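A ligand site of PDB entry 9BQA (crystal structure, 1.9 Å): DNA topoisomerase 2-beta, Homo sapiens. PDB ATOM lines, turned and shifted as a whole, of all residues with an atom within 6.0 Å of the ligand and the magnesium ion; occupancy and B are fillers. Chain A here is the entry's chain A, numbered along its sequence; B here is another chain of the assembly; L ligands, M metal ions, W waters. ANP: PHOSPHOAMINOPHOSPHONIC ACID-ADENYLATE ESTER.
The side-chain carboxylate of Glu 62 sits close to an oxygen (O1G) of the ligand. Residues that only touch the ligand: Ile 116 (3.2 Å), Gly 136 (3.5 Å), Ile 100 (3.5 Å), Tyr 9 of chain B (3.5 Å), Phe 117 (3.5 Å), Thr 122 (3.7 Å), Arg 73 (3.7 Å) and Thr 190 (3.8 Å). Hydrophobic or aromatic side chains within 4 Å of the ligand: Ile 100, Ile 116, Phe 117, Tyr 140, Ala 142 and Tyr 9 of chain B. Of the 32 residues printed, 24 come within 4 Å of the ligand. The nearest printed residue that does not touch the ligand is Ala 67 (4.04 Å).
NZ of Lys 353 is in hydrogen-bond range of O of Gly 135 (2.9 Å). O of Gly 139 sits close to NZ of Lys 143 (3.3 Å). The side-chain amino group (NZ) of Lys 143 lies within hydrogen-bond range of the backbone carbonyl oxygen (O) of Ile 116 (2.8 Å). OG1 of Thr 122 sits at hydrogen-bond distance from NZ of Lys 143. The backbone carbonyl oxygen (O) of Gly 136 lies close to the side-chain amide nitrogen (ND2) of Asn 125 (3.4 Å). The backbone NH (N) of Gly 136 sits at hydrogen-bond distance from the side-chain carboxylate (OD2) of Asp 69 (3.0 Å). The guanidinium group of Arg 73 sits at hydrogen-bond distance from the backbone carbonyl oxygen of Lys 98. The backbone carbonyl oxygen of Gly 99 sits at hydrogen-bond distance from the guanidinium group of Arg 73 (3.0 Å).
The magnesium ion is bound by O1G of the ligand, O2A of the ligand, O1B of the ligand, OD1 of Asn 66, water W9 and water W1.
Water W1 bridges OD2 of Asp 69 and N of Gly 136. Water W2 lies within hydrogen-bond range of the side-chain hydroxyl (OG1) of Thr 190, a nitrogen (N1) of the ligand, the backbone carbonyl oxygen (O) of Lys 98, the side-chain amide nitrogen (ND2) of Asn 95 and the side-chain amide nitrogen (ND2) of Asn 70. Water W4 lies within hydrogen-bond range of N3 of the ligand (2.8 Å), OH of Tyr 9 of chain B (2.8 Å) and NE of Arg 73 (3.1 Å). Water W5 bridges O of Asn 66 (2.9 Å) and N7 of the ligand (3.4 Å). Water W8 lies within hydrogen-bond range of the backbone carbonyl oxygen (O) of Ile 63, a nitrogen (N6) of the ligand and the backbone NH (N) of Ala 67. Water W10 lies within hydrogen-bond range of NZ of Lys 353 (2.8 Å) and OE1 of Glu 62 (2.8 Å).
The side-chain hydroxyl (OG) of Ser 123 lies within hydrogen-bond range of an oxygen (O2B) of the ligand, 2.6 Å away. NZ of Lys 353 lies within salt-bridge range of O3G of the ligand (2.6 Å). The side-chain amino group (NZ) of Lys 143 is in salt-bridge range of an oxygen (O1A) of the ligand (2.7 Å). N of Arg 137 sits at hydrogen-bond distance from O3G of the ligand (2.8 Å). The backbone NH (N) of Tyr 140 is in hydrogen-bond range of an oxygen (O2G) of the ligand (2.8 Å). O3' of the ligand is in hydrogen-bond range of N of Ser 124 (3.0 Å). OG of Ser 124 lies within hydrogen-bond range of O2' of the ligand. N of Gly 141 sits at hydrogen-bond distance from O2G of the ligand (2.8 Å). N of Asn 138 lies within hydrogen-bond range of O3G of the ligand, 2.9 Å away. The side-chain amide oxygen (OD1) of Asn 95 lies within hydrogen-bond range of a nitrogen (N6) of the ligand (2.9 Å). An oxygen (O2G) of the ligand is in hydrogen-bond range of the side-chain amide nitrogen of Gln 351 (3.0 Å). The backbone NH of Ala 142 sits at hydrogen-bond distance from an oxygen (O1A) of the ligand, 3.0 Å away. The backbone NH (N) of Gly 139 lies within hydrogen-bond range of an oxygen (O2G) of the ligand. ND2 of Asn 125 is in hydrogen-bond range of O2B of the ligand, 3.1 Å away. The side-chain amide oxygen (OD1) of Asn 70 lies close to a nitrogen (N1) of the ligand (3.3 Å).
The nearest printed residue that does not touch the magnesium ion is Glu 62 (4.04 Å).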
ATOM      1  N   GLU A  62     -11.146   1.992   8.087  1.00  0.00           N
ATOM      2  CA  GLU A  62     -10.794   2.705   9.304  1.00  0.00           C
ATOM      3  C   GLU A  62     -10.039   1.803  10.269  1.00  0.00           C
ATOM      4  O   GLU A  62      -9.037   2.206  10.873  1.00  0.00           O
ATOM      5  CB  GLU A  62     -12.054   3.255   9.991  1.00  0.00           C
ATOM      6  CG  GLU A  62     -12.760   4.371   9.253  1.00  0.00           C
ATOM      7  CD  GLU A  62     -11.961   5.658   9.173  1.00  0.00           C
ATOM      8  OE1 GLU A  62     -10.867   5.757   9.764  1.00  0.00           O
ATOM      9  OE2 GLU A  62     -12.457   6.593   8.493  1.00  0.00           O
ATOM     10  N   ILE A  63     -10.513   0.563  10.439  1.00  0.00           N
ATOM     11  CA  ILE A  63      -9.878  -0.374  11.363  1.00  0.00           C
ATOM     12  C   ILE A  63      -8.536  -0.840  10.820  1.00  0.00           C
ATOM     13  O   ILE A  63      -7.575  -1.025  11.566  1.00  0.00           O
ATOM     14  CB  ILE A  63     -10.834  -1.549  11.658  1.00  0.00           C
ATOM     15  CG1 ILE A  63     -12.169  -1.006  12.191  1.00  0.00           C
ATOM     16  CG2 ILE A  63     -10.209  -2.554  12.622  1.00  0.00           C
ATOM     17  CD1 ILE A  63     -12.035  -0.133  13.468  1.00  0.00           C
ATOM     18  N   VAL A  65      -6.423   0.860   8.770  1.00  0.00           N
ATOM     19  CA  VAL A  65      -5.447   1.941   8.918  1.00  0.00           C
ATOM     20  C   VAL A  65      -5.068   2.147  10.376  1.00  0.00           C
ATOM     21  O   VAL A  65      -3.919   2.449  10.694  1.00  0.00           O
ATOM     22  CB  VAL A  65      -6.000   3.247   8.296  1.00  0.00           C
ATOM     23  CG1 VAL A  65      -5.045   4.404   8.544  1.00  0.00           C
ATOM     24  CG2 VAL A  65      -6.237   3.064   6.796  1.00  0.00           C
ATOM     25  N   ASN A  66      -6.025   1.964  11.298  1.00  0.00           N
ATOM     26  CA  ASN A  66      -5.690   2.030  12.713  1.00  0.00           C
ATOM     27  C   ASN A  66      -4.646   0.976  13.084  1.00  0.00           C
ATOM     28  O   ASN A  66      -3.765   1.244  13.911  1.00  0.00           O
ATOM     29  CB  ASN A  66      -6.932   1.825  13.581  1.00  0.00           C
ATOM     30  CG  ASN A  66      -7.795   3.057  13.667  1.00  0.00           C
ATOM     31  OD1 ASN A  66      -7.387   4.151  13.274  1.00  0.00           O
ATOM     32  ND2 ASN A  66      -9.000   2.884  14.207  1.00  0.00           N
ATOM     33  N   ALA A  67      -4.751  -0.224  12.525  1.00  0.00           N
ATOM     34  CA  ALA A  67      -3.719  -1.234  12.761  1.00  0.00           C
ATOM     35  C   ALA A  67      -2.378  -0.771  12.195  1.00  0.00           C
ATOM     36  O   ALA A  67      -1.334  -0.899  12.853  1.00  0.00           O
ATOM     37  CB  ALA A  67      -4.138  -2.565  12.137  1.00  0.00           C
ATOM     38  N   ASP A  69      -1.398   2.231  11.800  1.00  0.00           N
ATOM     39  CA  ASP A  69      -0.935   3.339  12.636  1.00  0.00           C
ATOM     40  C   ASP A  69      -0.175   2.855  13.858  1.00  0.00           C
ATOM     41  O   ASP A  69       0.648   3.600  14.404  1.00  0.00           O
ATOM     42  CB  ASP A  69      -2.117   4.173  13.081  1.00  0.00           C
ATOM     43  CG  ASP A  69      -2.656   5.056  11.976  1.00  0.00           C
ATOM     44  OD1 ASP A  69      -1.928   5.228  10.966  1.00  0.00           O
ATOM     45  OD2 ASP A  69      -3.784   5.562  12.133  1.00  0.00           O
ATOM     46  N   ASN A  70      -0.458   1.635  14.327  1.00  0.00           N
ATOM     47  CA  ASN A  70       0.220   1.174  15.526  1.00  0.00           C
ATOM     48  C   ASN A  70       1.705   0.969  15.285  1.00  0.00           C
ATOM     49  O   ASN A  70       2.474   0.938  16.252  1.00  0.00           O
ATOM     50  CB  ASN A  70      -0.397  -0.121  16.055  1.00  0.00           C
ATOM     51  CG  ASN A  70      -0.144  -0.311  17.542  1.00  0.00           C
ATOM     52  OD1 ASN A  70      -0.548   0.520  18.346  1.00  0.00           O
ATOM     53  ND2 ASN A  70       0.538  -1.397  17.900  1.00  0.00           N
ATOM     54  N   ARG A  73       3.249   3.867  16.925  1.00  0.00           N
ATOM     55  CA  ARG A  73       3.317   3.778  18.376  1.00  0.00           C
ATOM     56  C   ARG A  73       4.400   2.808  18.823  1.00  0.00           C
ATOM     57  O   ARG A  73       5.024   3.003  19.873  1.00  0.00           O
ATOM     58  CB  ARG A  73       1.983   3.302  18.968  1.00  0.00           C
ATOM     59  CG  ARG A  73       0.877   4.310  19.074  1.00  0.00           C
ATOM     60  CD  ARG A  73      -0.341   3.657  19.765  1.00  0.00           C
ATOM     61  NE  ARG A  73      -0.146   3.449  21.202  1.00  0.00           N
ATOM     62  CZ  ARG A  73      -0.194   2.273  21.819  1.00  0.00           C
ATOM     63  NH1 ARG A  73      -0.439   1.147  21.175  1.00  0.00           N
ATOM     64  NH2 ARG A  73      -0.009   2.236  23.136  1.00  0.00           N
ATOM     65  N   ASN A  95      -3.337  -7.060  15.175  1.00  0.00           N
ATOM     66  CA  ASN A  95      -1.977  -6.547  15.019  1.00  0.00           C
ATOM     67  C   ASN A  95      -1.207  -6.841  16.306  1.00  0.00           C
ATOM     68  O   ASN A  95      -1.800  -6.996  17.378  1.00  0.00           O
ATOM     69  CB  ASN A  95      -1.977  -5.036  14.692  1.00  0.00           C
ATOM     70  CG  ASN A  95      -2.486  -4.166  15.832  1.00  0.00           C
ATOM     71  OD1 ASN A  95      -3.648  -3.778  15.873  1.00  0.00           O
ATOM     72  ND2 ASN A  95      -1.594  -3.839  16.764  1.00  0.00           N
ATOM     73  N   LYS A  98       2.711  -2.938  20.670  1.00  0.00           N
ATOM     74  CA  LYS A  98       2.102  -2.505  21.927  1.00  0.00           C
ATOM     75  C   LYS A  98       0.584  -2.474  21.830  1.00  0.00           C
ATOM     76  O   LYS A  98       0.014  -1.995  20.848  1.00  0.00           O
ATOM     77  CB  LYS A  98       2.628  -1.117  22.306  1.00  0.00           C
ATOM     78  CG  LYS A  98       2.349  -0.717  23.750  1.00  0.00           C
ATOM     79  CD  LYS A  98       3.156   0.517  24.158  1.00  0.00           C
ATOM     80  CE  LYS A  98       2.837   0.954  25.585  1.00  0.00           C
ATOM     81  NZ  LYS A  98       3.177  -0.083  26.593  1.00  0.00           N
ATOM     82  N   GLY A  99      -0.064  -3.014  22.857  1.00  0.00           N
ATOM     83  CA  GLY A  99      -1.504  -2.926  22.972  1.00  0.00           C
ATOM     84  C   GLY A  99      -1.924  -1.554  23.468  1.00  0.00           C
ATOM     85  O   GLY A  99      -1.134  -0.611  23.522  1.00  0.00           O
ATOM     86  N   ILE A 100      -3.194  -1.459  23.845  1.00  0.00           N
ATOM     87  CA  ILE A 100      -3.730  -0.211  24.384  1.00  0.00           C
ATOM     88  C   ILE A 100      -3.723  -0.290  25.904  1.00  0.00           C
ATOM     89  O   ILE A 100      -4.145  -1.317  26.460  1.00  0.00           O
ATOM     90  CB  ILE A 100      -5.140   0.057  23.842  1.00  0.00           C
ATOM     91  CG1 ILE A 100      -5.107   0.156  22.320  1.00  0.00           C
ATOM     92  CG2 ILE A 100      -5.711   1.332  24.450  1.00  0.00           C
ATOM     93  CD1 ILE A 100      -6.466   0.078  21.701  1.00  0.00           C
ATOM     94  N   ILE A 116     -11.839   5.234  23.753  1.00  0.00           N
ATOM     95  CA  ILE A 116     -11.428   5.556  22.402  1.00  0.00           C
ATOM     96  C   ILE A 116     -12.096   4.691  21.340  1.00  0.00           C
ATOM     97  O   ILE A 116     -11.978   5.002  20.149  1.00  0.00           O
ATOM     98  CB  ILE A 116      -9.899   5.489  22.272  1.00  0.00           C
ATOM     99  CG1 ILE A 116      -9.380   4.042  22.366  1.00  0.00           C
ATOM    100  CG2 ILE A 116      -9.240   6.357  23.361  1.00  0.00           C
ATOM    101  CD1 ILE A 116      -7.842   3.946  22.437  1.00  0.00           C
ATOM    102  N   PHE A 117     -12.802   3.626  21.731  1.00  0.00           N
ATOM    103  CA  PHE A 117     -13.625   2.879  20.793  1.00  0.00           C
ATOM    104  C   PHE A 117     -15.111   3.110  20.979  1.00  0.00           C
ATOM    105  O   PHE A 117     -15.899   2.795  20.068  1.00  0.00           O
ATOM    106  CB  PHE A 117     -13.323   1.377  20.889  1.00  0.00           C
ATOM    107  CG  PHE A 117     -12.001   0.994  20.288  1.00  0.00           C
ATOM    108  CD1 PHE A 117     -11.886   0.770  18.931  1.00  0.00           C
ATOM    109  CD2 PHE A 117     -10.874   0.896  21.085  1.00  0.00           C
ATOM    110  CE1 PHE A 117     -10.666   0.438  18.372  1.00  0.00           C
ATOM    111  CE2 PHE A 117      -9.654   0.565  20.527  1.00  0.00           C
ATOM    112  CZ  PHE A 117      -9.553   0.338  19.173  1.00  0.00           C
ATOM    113  N   THR A 122     -12.378  11.036  20.180  1.00  0.00           N
ATOM    114  CA  THR A 122     -11.330  10.568  21.074  1.00  0.00           C
ATOM    115  C   THR A 122     -10.179  10.040  20.235  1.00  0.00           C
ATOM    116  O   THR A 122     -10.391   9.292  19.281  1.00  0.00           O
ATOM    117  CB  THR A 122     -11.853   9.461  21.999  1.00  0.00           C
ATOM    118  OG1 THR A 122     -12.438   8.424  21.197  1.00  0.00           O
ATOM    119  CG2 THR A 122     -12.904  10.000  22.941  1.00  0.00           C
ATOM    120  N   SER A 123      -8.949  10.407  20.607  1.00  0.00           N
ATOM    121  CA  SER A 123      -7.805  10.147  19.738  1.00  0.00           C
ATOM    122  C   SER A 123      -6.516  10.329  20.521  1.00  0.00           C
ATOM    123  O   SER A 123      -6.466  11.045  21.517  1.00  0.00           O
ATOM    124  CB  SER A 123      -7.814  11.096  18.523  1.00  0.00           C
ATOM    125  OG  SER A 123      -6.767  10.806  17.622  1.00  0.00           O
ATOM    126  N   SER A 124      -5.469   9.676  20.029  1.00  0.00           N
ATOM    127  CA  SER A 124      -4.105   9.970  20.454  1.00  0.00           C
ATOM    128  C   SER A 124      -3.406  10.887  19.455  1.00  0.00           C
ATOM    129  O   SER A 124      -2.202  11.141  19.609  1.00  0.00           O
ATOM    130  CB  SER A 124      -3.310   8.679  20.634  1.00  0.00           C
ATOM    131  OG  SER A 124      -3.223   7.964  19.416  1.00  0.00           O
ATOM    132  N   ASN A 125      -4.124  11.392  18.450  1.00  0.00           N
ATOM    133  CA  ASN A 125      -3.546  12.191  17.371  1.00  0.00           C
ATOM    134  C   ASN A 125      -4.034  13.629  17.380  1.00  0.00           C
ATOM    135  O   ASN A 125      -4.026  14.283  16.328  1.00  0.00           O
ATOM    136  CB  ASN A 125      -3.862  11.532  16.021  1.00  0.00           C
ATOM    137  CG  ASN A 125      -3.170  10.199  15.844  1.00  0.00           C
ATOM    138  OD1 ASN A 125      -1.952  10.132  15.769  1.00  0.00           O
ATOM    139  ND2 ASN A 125      -3.945   9.131  15.759  1.00  0.00           N
ATOM    140  N   GLY A 135      -2.002   7.699   9.896  1.00  0.00           N
ATOM    141  CA  GLY A 135      -3.172   8.096   9.129  1.00  0.00           C
ATOM    142  C   GLY A 135      -4.255   8.697   9.972  1.00  0.00           C
ATOM    143  O   GLY A 135      -5.049   9.498   9.475  1.00  0.00           O
ATOM    144  N   GLY A 136      -4.268   8.367  11.263  1.00  0.00           N
ATOM    145  CA  GLY A 136      -5.334   8.828  12.137  1.00  0.00           C
ATOM    146  C   GLY A 136      -5.192  10.300  12.427  1.00  0.00           C
ATOM    147  O   GLY A 136      -4.099  10.782  12.757  1.00  0.00           O
ATOM    148  N   ARG A 137      -6.287  11.025  12.324  1.00  0.00           N
ATOM    149  CA  ARG A 137      -6.243  12.452  12.598  1.00  0.00           C
ATOM    150  C   ARG A 137      -7.420  12.998  13.396  1.00  0.00           C
ATOM    151  O   ARG A 137      -7.218  13.948  14.152  1.00  0.00           O
ATOM    152  CB  ARG A 137      -6.127  13.212  11.268  1.00  0.00           C
ATOM    153  CG  ARG A 137      -4.838  12.899  10.492  1.00  0.00           C
ATOM    154  CD  ARG A 137      -3.623  13.499  11.188  1.00  0.00           C
ATOM    155  NE  ARG A 137      -3.696  14.949  11.162  1.00  0.00           N
ATOM    156  CZ  ARG A 137      -3.032  15.755  11.979  1.00  0.00           C
ATOM    157  NH1 ARG A 137      -2.138  15.281  12.834  1.00  0.00           N
ATOM    158  NH2 ARG A 137      -3.262  17.064  11.930  1.00  0.00           N
ATOM    159  N   ASN A 138      -8.615  12.396  13.325  1.00  0.00           N
ATOM    160  CA  ASN A 138      -9.846  13.070  13.719  1.00  0.00           C
ATOM    161  C   ASN A 138     -10.543  12.500  14.942  1.00  0.00           C
ATOM    162  O   ASN A 138     -11.386  13.184  15.526  1.00  0.00           O
ATOM    163  CB  ASN A 138     -10.835  13.058  12.541  1.00  0.00           C
ATOM    164  CG  ASN A 138     -10.300  13.755  11.312  1.00  0.00           C
ATOM    165  OD1 ASN A 138      -9.633  14.780  11.407  1.00  0.00           O
ATOM    166  ND2 ASN A 138     -10.607  13.219  10.144  1.00  0.00           N
ATOM    167  N   GLY A 139     -10.223  11.260  15.341  1.00  0.00           N
ATOM    168  CA  GLY A 139     -10.888  10.667  16.486  1.00  0.00           C
ATOM    169  C   GLY A 139     -12.275  10.142  16.220  1.00  0.00           C
ATOM    170  O   GLY A 139     -13.086  10.073  17.155  1.00  0.00           O
ATOM    171  N   TYR A 140     -12.569   9.746  14.979  1.00  0.00           N
ATOM    172  CA  TYR A 140     -13.855   9.163  14.587  1.00  0.00           C
ATOM    173  C   TYR A 140     -13.779   7.697  14.156  1.00  0.00           C
ATOM    174  O   TYR A 140     -14.705   6.929  14.432  1.00  0.00           O
ATOM    175  CB  TYR A 140     -14.451   9.940  13.402  1.00  0.00           C
ATOM    176  CG  TYR A 140     -15.312  11.133  13.709  1.00  0.00           C
ATOM    177  CD1 TYR A 140     -16.516  10.992  14.391  1.00  0.00           C
ATOM    178  CD2 TYR A 140     -14.956  12.402  13.278  1.00  0.00           C
ATOM    179  CE1 TYR A 140     -17.316  12.098  14.673  1.00  0.00           C
ATOM    180  CE2 TYR A 140     -15.745  13.502  13.543  1.00  0.00           C
ATOM    181  CZ  TYR A 140     -16.930  13.355  14.238  1.00  0.00           C
ATOM    182  OH  TYR A 140     -17.718  14.455  14.503  1.00  0.00           O
ATOM    183  N   GLY A 141     -12.741   7.322  13.423  1.00  0.00           N
ATOM    184  CA  GLY A 141     -12.752   6.108  12.635  1.00  0.00           C
ATOM    185  C   GLY A 141     -13.320   4.873  13.305  1.00  0.00           C
ATOM    186  O   GLY A 141     -14.254   4.245  12.778  1.00  0.00           O
ATOM    187  N   ALA A 142     -12.766   4.516  14.452  1.00  0.00           N
ATOM    188  CA  ALA A 142     -13.157   3.288  15.132  1.00  0.00           C
ATOM    189  C   ALA A 142     -14.607   3.354  15.605  1.00  0.00           C
ATOM    190  O   ALA A 142     -15.317   2.345  15.599  1.00  0.00           O
ATOM    191  CB  ALA A 142     -12.239   3.025  16.311  1.00  0.00           C
ATOM    192  N   LYS A 143     -15.048   4.538  16.063  1.00  0.00           N
ATOM    193  CA  LYS A 143     -16.427   4.689  16.487  1.00  0.00           C
ATOM    194  C   LYS A 143     -17.376   4.551  15.296  1.00  0.00           C
ATOM    195  O   LYS A 143     -18.471   4.003  15.428  1.00  0.00           O
ATOM    196  CB  LYS A 143     -16.612   6.040  17.181  1.00  0.00           C
ATOM    197  CG  LYS A 143     -16.193   6.072  18.659  1.00  0.00           C
ATOM    198  CD  LYS A 143     -14.679   5.999  18.840  1.00  0.00           C
ATOM    199  CE  LYS A 143     -13.979   7.272  18.380  1.00  0.00           C
ATOM    200  NZ  LYS A 143     -12.479   7.197  18.564  1.00  0.00           N
ATOM    201  N   THR A 190      -3.677  -6.197  19.624  1.00  0.00           N
ATOM    202  CA  THR A 190      -5.036  -5.671  19.571  1.00  0.00           C
ATOM    203  C   THR A 190      -5.750  -6.417  18.454  1.00  0.00           C
ATOM    204  O   THR A 190      -5.188  -6.608  17.373  1.00  0.00           O
ATOM    205  CB  THR A 190      -5.040  -4.162  19.325  1.00  0.00           C
ATOM    206  OG1 THR A 190      -4.440  -3.508  20.453  1.00  0.00           O
ATOM    207  CG2 THR A 190      -6.462  -3.643  19.136  1.00  0.00           C
ATOM    208  N   ILE A 192      -9.581  -6.285  16.641  1.00  0.00           N
ATOM    209  CA  ILE A 192     -10.904  -5.705  16.454  1.00  0.00           C
ATOM    210  C   ILE A 192     -11.710  -6.691  15.615  1.00  0.00           C
ATOM    211  O   ILE A 192     -11.307  -7.032  14.496  1.00  0.00           O
ATOM    212  CB  ILE A 192     -10.826  -4.334  15.750  1.00  0.00           C
ATOM    213  CG1 ILE A 192      -9.833  -3.429  16.473  1.00  0.00           C
ATOM    214  CG2 ILE A 192     -12.228  -3.734  15.653  1.00  0.00           C
ATOM    215  CD1 ILE A 192     -10.129  -3.200  17.908  1.00  0.00           C
ATOM    216  N   GLN A 351     -13.587  12.947   6.113  1.00  0.00           N
ATOM    217  CA  GLN A 351     -13.165  11.846   6.975  1.00  0.00           C
ATOM    218  C   GLN A 351     -12.703  10.649   6.150  1.00  0.00           C
ATOM    219  O   GLN A 351     -11.900   9.847   6.620  1.00  0.00           O
ATOM    220  CB  GLN A 351     -14.307  11.433   7.908  1.00  0.00           C
ATOM    221  CG  GLN A 351     -14.017  10.183   8.748  1.00  0.00           C
ATOM    222  CD  GLN A 351     -12.952  10.385   9.811  1.00  0.00           C
ATOM    223  OE1 GLN A 351     -12.715  11.495  10.266  1.00  0.00           O
ATOM    224  NE2 GLN A 351     -12.294   9.298  10.198  1.00  0.00           N
ATOM    225  N   LYS A 353     -10.850  10.651   3.551  1.00  0.00           N
ATOM    226  CA  LYS A 353      -9.410  10.835   3.304  1.00  0.00           C
ATOM    227  C   LYS A 353      -9.000  10.407   1.901  1.00  0.00           C
ATOM    228  O   LYS A 353      -7.908   9.895   1.671  1.00  0.00           O
ATOM    229  CB  LYS A 353      -8.584  10.104   4.364  1.00  0.00           C
ATOM    230  CG  LYS A 353      -8.709  10.721   5.742  1.00  0.00           C
ATOM    231  CD  LYS A 353      -8.028   9.888   6.795  1.00  0.00           C
ATOM    232  CE  LYS A 353      -8.512  10.263   8.183  1.00  0.00           C
ATOM    233  NZ  LYS A 353      -7.936   9.344   9.191  1.00  0.00           N
ATOM    234  N   TYR B   9      -4.272  10.143  25.324  1.00  0.00           N
ATOM    235  CA  TYR B   9      -5.636   9.898  24.865  1.00  0.00           C
ATOM    236  C   TYR B   9      -6.527  11.044  25.308  1.00  0.00           C
ATOM    237  O   TYR B   9      -6.792  11.222  26.502  1.00  0.00           O
ATOM    238  CB  TYR B   9      -6.140   8.569  25.414  1.00  0.00           C
ATOM    239  CG  TYR B   9      -5.265   7.416  24.995  1.00  0.00           C
ATOM    240  CD1 TYR B   9      -5.370   6.893  23.718  1.00  0.00           C
ATOM    241  CD2 TYR B   9      -4.324   6.887  25.856  1.00  0.00           C
ATOM    242  CE1 TYR B   9      -4.581   5.838  23.314  1.00  0.00           C
ATOM    243  CE2 TYR B   9      -3.526   5.823  25.457  1.00  0.00           C
ATOM    244  CZ  TYR B   9      -3.654   5.320  24.184  1.00  0.00           C
ATOM    245  OH  TYR B   9      -2.870   4.261  23.757  1.00  0.00           O
HETATM  246  PG  ANP L   1      -9.308   9.001  12.565  1.00  0.00           P
HETATM  247  O1G ANP L   1      -9.087   7.586  12.129  1.00  0.00           O
HETATM  248  O2G ANP L   1     -10.826   9.338  12.821  1.00  0.00           O
HETATM  249  O3G ANP L   1      -8.764  10.073  11.537  1.00  0.00           O
HETATM  250  PB  ANP L   1      -7.950   8.119  15.005  1.00  0.00           P
HETATM  251  O1B ANP L   1      -7.251   6.975  14.343  1.00  0.00           O
HETATM  252  O2B ANP L   1      -6.992   8.795  16.041  1.00  0.00           O
HETATM  253  N3B ANP L   1      -8.354   9.324  13.925  1.00  0.00           N
HETATM  254  PA  ANP L   1      -9.909   6.246  15.792  1.00  0.00           P
HETATM  255  O1A ANP L   1     -11.291   6.404  16.313  1.00  0.00           O
HETATM  256  O2A ANP L   1      -9.708   5.558  14.439  1.00  0.00           O
HETATM  257  O3A ANP L   1      -9.220   7.677  15.790  1.00  0.00           O
HETATM  258  O5' ANP L   1      -9.104   5.481  16.900  1.00  0.00           O
HETATM  259  C5' ANP L   1      -9.145   6.012  18.223  1.00  0.00           C
HETATM  260  C4' ANP L   1      -7.834   5.769  18.909  1.00  0.00           C
HETATM  261  O4' ANP L   1      -7.736   4.379  19.277  1.00  0.00           O
HETATM  262  C3' ANP L   1      -6.601   6.045  18.055  1.00  0.00           C
HETATM  263  O3' ANP L   1      -6.243   7.418  18.143  1.00  0.00           O
HETATM  264  C2' ANP L   1      -5.554   5.151  18.710  1.00  0.00           C
HETATM  265  O2' ANP L   1      -4.964   5.785  19.843  1.00  0.00           O
HETATM  266  C1' ANP L   1      -6.380   3.970  19.239  1.00  0.00           C
HETATM  267  N9  ANP L   1      -6.306   2.753  18.436  1.00  0.00           N
HETATM  268  C8  ANP L   1      -7.170   2.330  17.460  1.00  0.00           C
HETATM  269  N7  ANP L   1      -6.848   1.188  16.920  1.00  0.00           N
HETATM  270  C5  ANP L   1      -5.678   0.830  17.579  1.00  0.00           C
HETATM  271  C6  ANP L   1      -4.827  -0.291  17.459  1.00  0.00           C
HETATM  272  N6  ANP L   1      -5.023  -1.286  16.588  1.00  0.00           N
HETATM  273  N1  ANP L   1      -3.754  -0.348  18.280  1.00  0.00           N
HETATM  274  C2  ANP L   1      -3.550   0.654  19.152  1.00  0.00           C
HETATM  275  N3  ANP L   1      -4.285   1.750  19.353  1.00  0.00           N
HETATM  276  C4  ANP L   1      -5.341   1.780  18.525  1.00  0.00           C
HETATM  277 MG    MG M   1      -8.371   5.977  12.935  1.00  0.00          MG
HETATM  278  O   HOH W   1      -6.771   5.966  11.436  1.00  0.00           O
HETATM  279  O   HOH W   2      -2.316  -2.456  19.303  1.00  0.00           O
HETATM  280  O   HOH W   3      -1.878   3.190  17.448  1.00  0.00           O
HETATM  281  O   HOH W   4      -3.234   3.698  21.021  1.00  0.00           O
HETATM  282  O   HOH W   5      -4.258   3.194  15.934  1.00  0.00           O
HETATM  283  O   HOH W   6      -8.976   0.061  15.419  1.00  0.00           O
HETATM  284  O   HOH W   7      -4.763   5.585  14.733  1.00  0.00           O
HETATM  285  O   HOH W   8      -7.125  -1.890  14.300  1.00  0.00           O
HETATM  286  O   HOH W   9      -9.436   4.746  11.571  1.00  0.00           O
HETATM  287  O   HOH W  10      -8.348   6.614   8.911  1.00  0.00           O
